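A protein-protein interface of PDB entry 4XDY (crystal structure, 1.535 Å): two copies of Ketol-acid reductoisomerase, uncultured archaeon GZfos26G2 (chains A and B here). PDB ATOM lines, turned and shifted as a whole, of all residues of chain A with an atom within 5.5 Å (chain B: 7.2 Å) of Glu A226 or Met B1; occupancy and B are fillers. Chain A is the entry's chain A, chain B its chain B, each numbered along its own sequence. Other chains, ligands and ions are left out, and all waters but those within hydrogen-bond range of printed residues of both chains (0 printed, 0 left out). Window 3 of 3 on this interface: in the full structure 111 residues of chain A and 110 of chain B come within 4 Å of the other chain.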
ATOM      1  N   PRO A 224       5.088 -21.496 -22.974  1.00  0.00           N
ATOM      2  CA  PRO A 224       4.527 -21.842 -24.305  1.00  0.00           C
ATOM      3  C   PRO A 224       3.564 -23.036 -24.151  1.00  0.00           C
ATOM      4  O   PRO A 224       3.828 -23.939 -23.363  1.00  0.00           O
ATOM      5  CB  PRO A 224       5.741 -22.300 -25.086  1.00  0.00           C
ATOM      6  CG  PRO A 224       6.903 -21.639 -24.454  1.00  0.00           C
ATOM      7  CD  PRO A 224       6.558 -21.392 -23.019  1.00  0.00           C
ATOM      8  N   PRO A 225       2.441 -23.003 -24.855  1.00  0.00           N
ATOM      9  CA  PRO A 225       1.547 -24.124 -24.811  1.00  0.00           C
ATOM     10  C   PRO A 225       2.134 -25.449 -25.225  1.00  0.00           C
ATOM     11  O   PRO A 225       1.696 -26.497 -24.676  1.00  0.00           O
ATOM     12  CB  PRO A 225       0.340 -23.660 -25.711  1.00  0.00           C
ATOM     13  CG  PRO A 225       0.975 -22.711 -26.685  1.00  0.00           C
ATOM     14  CD  PRO A 225       2.050 -22.005 -25.909  1.00  0.00           C
ATOM     15  N   GLU A 226       3.135 -25.474 -26.107  1.00  0.00           N
ATOM     16  CA  GLU A 226       3.775 -26.741 -26.429  1.00  0.00           C
ATOM     17  C   GLU A 226       4.495 -27.358 -25.200  1.00  0.00           C
ATOM     18  O   GLU A 226       4.491 -28.577 -24.971  1.00  0.00           O
ATOM     19  CB  GLU A 226       4.772 -26.546 -27.544  1.00  0.00           C
ATOM     20  CG  GLU A 226       4.118 -26.091 -28.860  1.00  0.00           C
ATOM     21  CD  GLU A 226       3.815 -24.633 -28.923  1.00  0.00           C
ATOM     22  OE1 GLU A 226       4.209 -23.777 -28.099  1.00  0.00           O
ATOM     23  OE2 GLU A 226       3.122 -24.355 -29.918  1.00  0.00           O
ATOM     24  N   MET A 227       5.105 -26.463 -24.433  1.00  0.00           N
ATOM     25  CA  MET A 227       5.797 -26.852 -23.174  1.00  0.00           C
ATOM     26  C   MET A 227       4.820 -27.388 -22.132  1.00  0.00           C
ATOM     27  O   MET A 227       5.024 -28.446 -21.577  1.00  0.00           O
ATOM     28  CB  MET A 227       6.615 -25.669 -22.723  1.00  0.00           C
ATOM     29  CG  MET A 227       7.545 -25.964 -21.546  1.00  0.00           C
ATOM     30  SD  MET A 227       8.398 -24.469 -21.014  1.00  0.00           S
ATOM     31  CE  MET A 227       9.433 -24.193 -22.453  1.00  0.00           C
ATOM     32  N   ALA A 228       3.698 -26.680 -21.933  1.00  0.00           N
ATOM     33  CA  ALA A 228       2.628 -27.097 -21.074  1.00  0.00           C
ATOM     34  C   ALA A 228       2.040 -28.384 -21.486  1.00  0.00           C
ATOM     35  O   ALA A 228       1.766 -29.251 -20.671  1.00  0.00           O
ATOM     36  CB  ALA A 228       1.576 -26.017 -20.962  1.00  0.00           C
ATOM     37  N   TYR A 229       1.903 -28.619 -22.797  1.00  0.00           N
ATOM     38  CA  TYR A 229       1.486 -29.955 -23.268  1.00  0.00           C
ATOM     39  C   TYR A 229       2.386 -31.126 -22.958  1.00  0.00           C
ATOM     40  O   TYR A 229       1.921 -32.153 -22.498  1.00  0.00           O
ATOM     41  CB  TYR A 229       1.148 -29.924 -24.819  1.00  0.00           C
ATOM     42  CG  TYR A 229       0.666 -31.279 -25.274  1.00  0.00           C
ATOM     43  CD1 TYR A 229       1.497 -32.208 -25.831  1.00  0.00           C
ATOM     44  CD2 TYR A 229      -0.669 -31.563 -25.293  1.00  0.00           C
ATOM     45  CE1 TYR A 229       1.060 -33.482 -26.174  1.00  0.00           C
ATOM     46  CE2 TYR A 229      -1.130 -32.783 -25.656  1.00  0.00           C
ATOM     47  CZ  TYR A 229      -0.303 -33.727 -26.094  1.00  0.00           C
ATOM     48  OH  TYR A 229      -0.827 -34.938 -26.445  1.00  0.00           O
ATOM     49  N   PHE A 230       3.692 -30.988 -23.202  1.00  0.00           N
ATOM     50  CA  PHE A 230       4.598 -32.052 -22.977  1.00  0.00           C
ATOM     51  C   PHE A 230       4.653 -32.343 -21.451  1.00  0.00           C
ATOM     52  O   PHE A 230       4.722 -33.482 -21.025  1.00  0.00           O
ATOM     53  CB  PHE A 230       5.964 -31.679 -23.429  1.00  0.00           C
ATOM     54  CG  PHE A 230       6.162 -31.716 -24.971  1.00  0.00           C
ATOM     55  CD1 PHE A 230       5.555 -32.715 -25.741  1.00  0.00           C
ATOM     56  CD2 PHE A 230       6.953 -30.819 -25.584  1.00  0.00           C
ATOM     57  CE1 PHE A 230       5.770 -32.809 -27.138  1.00  0.00           C
ATOM     58  CE2 PHE A 230       7.152 -30.850 -26.970  1.00  0.00           C
ATOM     59  CZ  PHE A 230       6.566 -31.851 -27.707  1.00  0.00           C
ATOM     60  N   GLU A 231       4.663 -31.292 -20.660  1.00  0.00           N
ATOM     61  CA  GLU A 231       4.749 -31.440 -19.189  1.00  0.00           C
ATOM     62  C   GLU A 231       3.484 -32.040 -18.607  1.00  0.00           C
ATOM     63  O   GLU A 231       3.584 -32.863 -17.716  1.00  0.00           O
ATOM     64  CB  GLU A 231       5.002 -30.102 -18.526  1.00  0.00           C
ATOM     65  CG  GLU A 231       5.182 -30.148 -17.030  1.00  0.00           C
ATOM     66  CD  GLU A 231       6.458 -30.797 -16.591  1.00  0.00           C
ATOM     67  OE1 GLU A 231       7.492 -30.694 -17.264  1.00  0.00           O
ATOM     68  OE2 GLU A 231       6.465 -31.483 -15.544  1.00  0.00           O
ATOM     69  N   VAL A 321      -3.332 -27.504 -29.711  1.00  0.00           N
ATOM     70  CA  VAL A 321      -1.874 -27.651 -29.726  1.00  0.00           C
ATOM     71  C   VAL A 321      -1.463 -29.092 -29.633  1.00  0.00           C
ATOM     72  O   VAL A 321      -0.546 -29.553 -30.326  1.00  0.00           O
ATOM     73  CB  VAL A 321      -1.221 -26.807 -28.636  1.00  0.00           C
ATOM     74  CG1 VAL A 321       0.300 -26.970 -28.638  1.00  0.00           C
ATOM     75  CG2 VAL A 321      -1.570 -25.344 -28.860  1.00  0.00           C
ATOM     76  N   GLU A 324      -1.629 -30.757 -33.027  1.00  0.00           N
ATOM     77  CA  GLU A 324      -0.542 -30.255 -33.904  1.00  0.00           C
ATOM     78  C   GLU A 324       0.742 -30.973 -33.519  1.00  0.00           C
ATOM     79  O   GLU A 324       1.480 -31.505 -34.358  1.00  0.00           O
ATOM     80  CB  GLU A 324      -0.337 -28.725 -33.702  1.00  0.00           C
ATOM     81  CG  GLU A 324      -1.482 -27.798 -34.105  1.00  0.00           C
ATOM     82  CD  GLU A 324      -1.248 -26.268 -33.869  1.00  0.00           C
ATOM     83  OE1 GLU A 324      -0.607 -25.778 -32.854  1.00  0.00           O
ATOM     84  OE2 GLU A 324      -1.772 -25.527 -34.748  1.00  0.00           O
ATOM     85  N   ILE A 325       0.978 -31.080 -32.179  1.00  0.00           N
ATOM     86  CA  ILE A 325       2.180 -31.811 -31.700  1.00  0.00           C
ATOM     87  C   ILE A 325       2.221 -33.272 -32.094  1.00  0.00           C
ATOM     88  O   ILE A 325       3.249 -33.799 -32.571  1.00  0.00           O
ATOM     89  CB  ILE A 325       2.323 -31.642 -30.150  1.00  0.00           C
ATOM     90  CG1 ILE A 325       2.645 -30.206 -29.777  1.00  0.00           C
ATOM     91  CG2 ILE A 325       3.314 -32.624 -29.560  1.00  0.00           C
ATOM     92  CD1 ILE A 325       2.655 -29.876 -28.299  1.00  0.00           C
ATOM     93  N   MET B   1       5.156 -21.696 -29.835  1.00  0.00           N
ATOM     94  CA  MET B   1       6.553 -21.720 -30.355  1.00  0.00           C
ATOM     95  C   MET B   1       6.988 -22.962 -31.152  1.00  0.00           C
ATOM     96  O   MET B   1       6.449 -24.023 -30.970  1.00  0.00           O
ATOM     97  CB  MET B   1       7.463 -21.657 -29.174  1.00  0.00           C
ATOM     98  CG  MET B   1       7.342 -22.907 -28.315  1.00  0.00           C
ATOM     99  SD  MET B   1       8.659 -23.198 -27.174  1.00  0.00           S
ATOM    100  CE  MET B   1      10.027 -22.562 -28.149  1.00  0.00           C
ATOM    101  N   GLU B   2       8.072 -22.832 -31.902  1.00  0.00           N
ATOM    102  CA  GLU B   2       8.507 -23.852 -32.787  1.00  0.00           C
ATOM    103  C   GLU B   2       9.102 -25.116 -32.099  1.00  0.00           C
ATOM    104  O   GLU B   2       9.726 -25.021 -31.062  1.00  0.00           O
ATOM    105  CB  GLU B   2       9.471 -23.212 -33.763  1.00  0.00           C
ATOM    106  CG  GLU B   2      10.952 -23.462 -33.539  1.00  0.00           C
ATOM    107  CD  GLU B   2      11.871 -22.657 -34.471  1.00  0.00           C
ATOM    108  OE1 GLU B   2      11.299 -21.947 -35.361  1.00  0.00           O
ATOM    109  OE2 GLU B   2      13.155 -22.722 -34.306  1.00  0.00           O
ATOM    110  N   ILE B   3       8.862 -26.268 -32.688  1.00  0.00           N
ATOM    111  CA  ILE B   3       9.302 -27.565 -32.184  1.00  0.00           C
ATOM    112  C   ILE B   3      10.303 -28.123 -33.171  1.00  0.00           C
ATOM    113  O   ILE B   3      10.021 -28.180 -34.398  1.00  0.00           O
ATOM    114  CB  ILE B   3       8.164 -28.561 -32.084  1.00  0.00           C
ATOM    115  CG1 ILE B   3       7.012 -28.035 -31.233  1.00  0.00           C
ATOM    116  CG2 ILE B   3       8.678 -29.928 -31.618  1.00  0.00           C
ATOM    117  CD1 ILE B   3       5.724 -28.807 -31.381  1.00  0.00           C
ATOM    118  N   LEU B   4      11.495 -28.457 -32.719  1.00  0.00           N
ATOM    119  CA  LEU B   4      12.521 -29.016 -33.566  1.00  0.00           C
ATOM    120  C   LEU B   4      12.461 -30.534 -33.603  1.00  0.00           C
ATOM    121  O   LEU B   4      12.264 -31.199 -32.579  1.00  0.00           O
ATOM    122  CB  LEU B   4      13.874 -28.573 -33.113  1.00  0.00           C
ATOM    123  CG  LEU B   4      14.089 -27.089 -32.911  1.00  0.00           C
ATOM    124  CD1 LEU B   4      15.508 -27.000 -32.458  1.00  0.00           C
ATOM    125  CD2 LEU B   4      13.950 -26.302 -34.220  1.00  0.00           C
ATOM    126  N   PRO B 152       9.896 -36.143 -25.535  1.00  0.00           N
ATOM    127  CA  PRO B 152      10.157 -34.744 -25.739  1.00  0.00           C
ATOM    128  C   PRO B 152      11.221 -34.177 -24.848  1.00  0.00           C
ATOM    129  O   PRO B 152      11.490 -34.720 -23.732  1.00  0.00           O
ATOM    130  CB  PRO B 152       8.802 -34.051 -25.409  1.00  0.00           C
ATOM    131  CG  PRO B 152       7.826 -35.198 -25.388  1.00  0.00           C
ATOM    132  CD  PRO B 152       8.542 -36.394 -24.985  1.00  0.00           C
ATOM    133  N   LEU B 154      13.592 -30.315 -23.679  1.00  0.00           N
ATOM    134  CA  LEU B 154      13.794 -28.919 -23.633  1.00  0.00           C
ATOM    135  C   LEU B 154      15.319 -28.686 -23.637  1.00  0.00           C
ATOM    136  O   LEU B 154      16.096 -29.367 -22.951  1.00  0.00           O
ATOM    137  CB  LEU B 154      13.189 -28.313 -22.389  1.00  0.00           C
ATOM    138  CG  LEU B 154      11.758 -27.759 -22.376  1.00  0.00           C
ATOM    139  CD1 LEU B 154      10.815 -28.743 -22.936  1.00  0.00           C
ATOM    140  CD2 LEU B 154      11.297 -27.408 -20.965  1.00  0.00           C
ATOM    141  N   ILE B 183      11.715 -31.165 -29.736  1.00  0.00           N
ATOM    142  CA  ILE B 183      12.567 -30.363 -28.847  1.00  0.00           C
ATOM    143  C   ILE B 183      12.064 -28.924 -28.839  1.00  0.00           C
ATOM    144  O   ILE B 183      11.798 -28.314 -29.929  1.00  0.00           O
ATOM    145  CB  ILE B 183      14.072 -30.446 -29.286  1.00  0.00           C
ATOM    146  CG1 ILE B 183      14.563 -31.877 -29.087  1.00  0.00           C
ATOM    147  CG2 ILE B 183      14.855 -29.293 -28.681  1.00  0.00           C
ATOM    148  CD1 ILE B 183      14.654 -32.364 -27.704  1.00  0.00           C
ATOM    149  N   LEU B 184      12.011 -28.315 -27.678  1.00  0.00           N
ATOM    150  CA  LEU B 184      11.695 -26.896 -27.502  1.00  0.00           C
ATOM    151  C   LEU B 184      12.913 -26.228 -26.938  1.00  0.00           C
ATOM    152  O   LEU B 184      13.529 -26.699 -25.947  1.00  0.00           O
ATOM    153  CB  LEU B 184      10.547 -26.692 -26.492  1.00  0.00           C
ATOM    154  CG  LEU B 184       9.277 -27.421 -26.749  1.00  0.00           C
ATOM    155  CD1 LEU B 184       8.244 -27.127 -25.701  1.00  0.00           C
ATOM    156  CD2 LEU B 184       8.727 -26.906 -28.094  1.00  0.00           C
ATOM    157  N   GLU B 185      13.279 -25.089 -27.482  1.00  0.00           N
ATOM    158  CA  GLU B 185      14.412 -24.335 -26.932  1.00  0.00           C
ATOM    159  C   GLU B 185      13.885 -23.355 -25.909  1.00  0.00           C
ATOM    160  O   GLU B 185      12.799 -22.767 -26.069  1.00  0.00           O
ATOM    161  CB  GLU B 185      15.205 -23.588 -28.036  1.00  0.00           C
ATOM    162  CG  GLU B 185      15.748 -24.509 -29.067  1.00  0.00           C
ATOM    163  CD  GLU B 185      16.797 -23.828 -29.931  1.00  0.00           C
ATOM    164  OE1 GLU B 185      16.450 -23.527 -31.097  1.00  0.00           O
ATOM    165  OE2 GLU B 185      17.904 -23.539 -29.430  1.00  0.00           O
ATOM    166  N   CYS B 186      14.595 -23.192 -24.794  1.00  0.00           N
ATOM    167  CA  CYS B 186      14.100 -22.376 -23.703  1.00  0.00           C
ATOM    168  C   CYS B 186      15.274 -21.908 -22.863  1.00  0.00           C
ATOM    169  O   CYS B 186      16.399 -22.167 -23.206  1.00  0.00           O
ATOM    170  CB  CYS B 186      13.059 -23.145 -22.855  1.00  0.00           C
ATOM    171  SG  CYS B 186      13.785 -24.594 -22.005  1.00  0.00           S
ATOM    172  N   GLN B 190      13.252 -21.201 -17.262  1.00  0.00           N
ATOM    173  CA  GLN B 190      11.986 -21.670 -17.721  1.00  0.00           C
ATOM    174  C   GLN B 190      11.774 -23.134 -17.483  1.00  0.00           C
ATOM    175  O   GLN B 190      10.675 -23.576 -17.115  1.00  0.00           O
ATOM    176  CB  GLN B 190      11.789 -21.419 -19.214  1.00  0.00           C
ATOM    177  CG  GLN B 190      11.450 -20.037 -19.566  1.00  0.00           C
ATOM    178  CD  GLN B 190      11.293 -19.997 -21.093  1.00  0.00           C
ATOM    179  OE1 GLN B 190      12.276 -20.130 -21.825  1.00  0.00           O
ATOM    180  NE2 GLN B 190      10.039 -19.942 -21.562  1.00  0.00           N
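Printed residues of chain B that touch a printed residue of chain A: Met B1, Ile B3, Pro B152, Leu B184 and Cys B186. Hydrophobic or aromatic side chains of chain B within 4 Å of the printed part of chain A: Met B1, Ile B3, Pro B152 and Leu B184. Along chain A the printed residues that touch a printed residue of chain B span positions 224 to 325. Among the printed residues, 8 pairs touch across the chains. Among the printed residues, no Asp or Glu carboxylate lies within 4 Å of a Lys or Arg side-chain nitrogen of the other chain.
Glu A226 touches just these residues of chain B: Met B1 (2.9 Å) and Leu B184 (3.8 Å). Printed residues of chain A within 4 Å of Met B1: Pro A224 and Glu A226. Of the printed residues of chain B, Ile A325 touches Ile B3. Of the printed residues of chain A, Pro B152 touches Phe A230 (3.4 Å). Of the printed residues of chain B, Pro A224 touches Met B1 (3.6 Å). Of the printed residues of chain A, Cys B186 touches Met A227. The nearest printed residue of chain A that does not touch Cys B186 is Pro A224 (6.5 Å).
Among the printed residues, pairs that only touch across the chains: Pro A224 with Met B1, Glu A226 with Leu B184, Met A227 with Leu B184, Met A227 with Cys B186, Phe A230 with Pro B152, Phe A230 with Leu B184 and Ile A325 with Ile B3.
No position is printed for both chains. Of the 8 pairs that touch across the chains among the printed residues, none has its exchanged pair printed and touching as well.
The backbone NH (N) of Met B1 lies within hydrogen-bond range of the side-chain carboxylate (OE1) of Glu A226 (2.9 Å).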
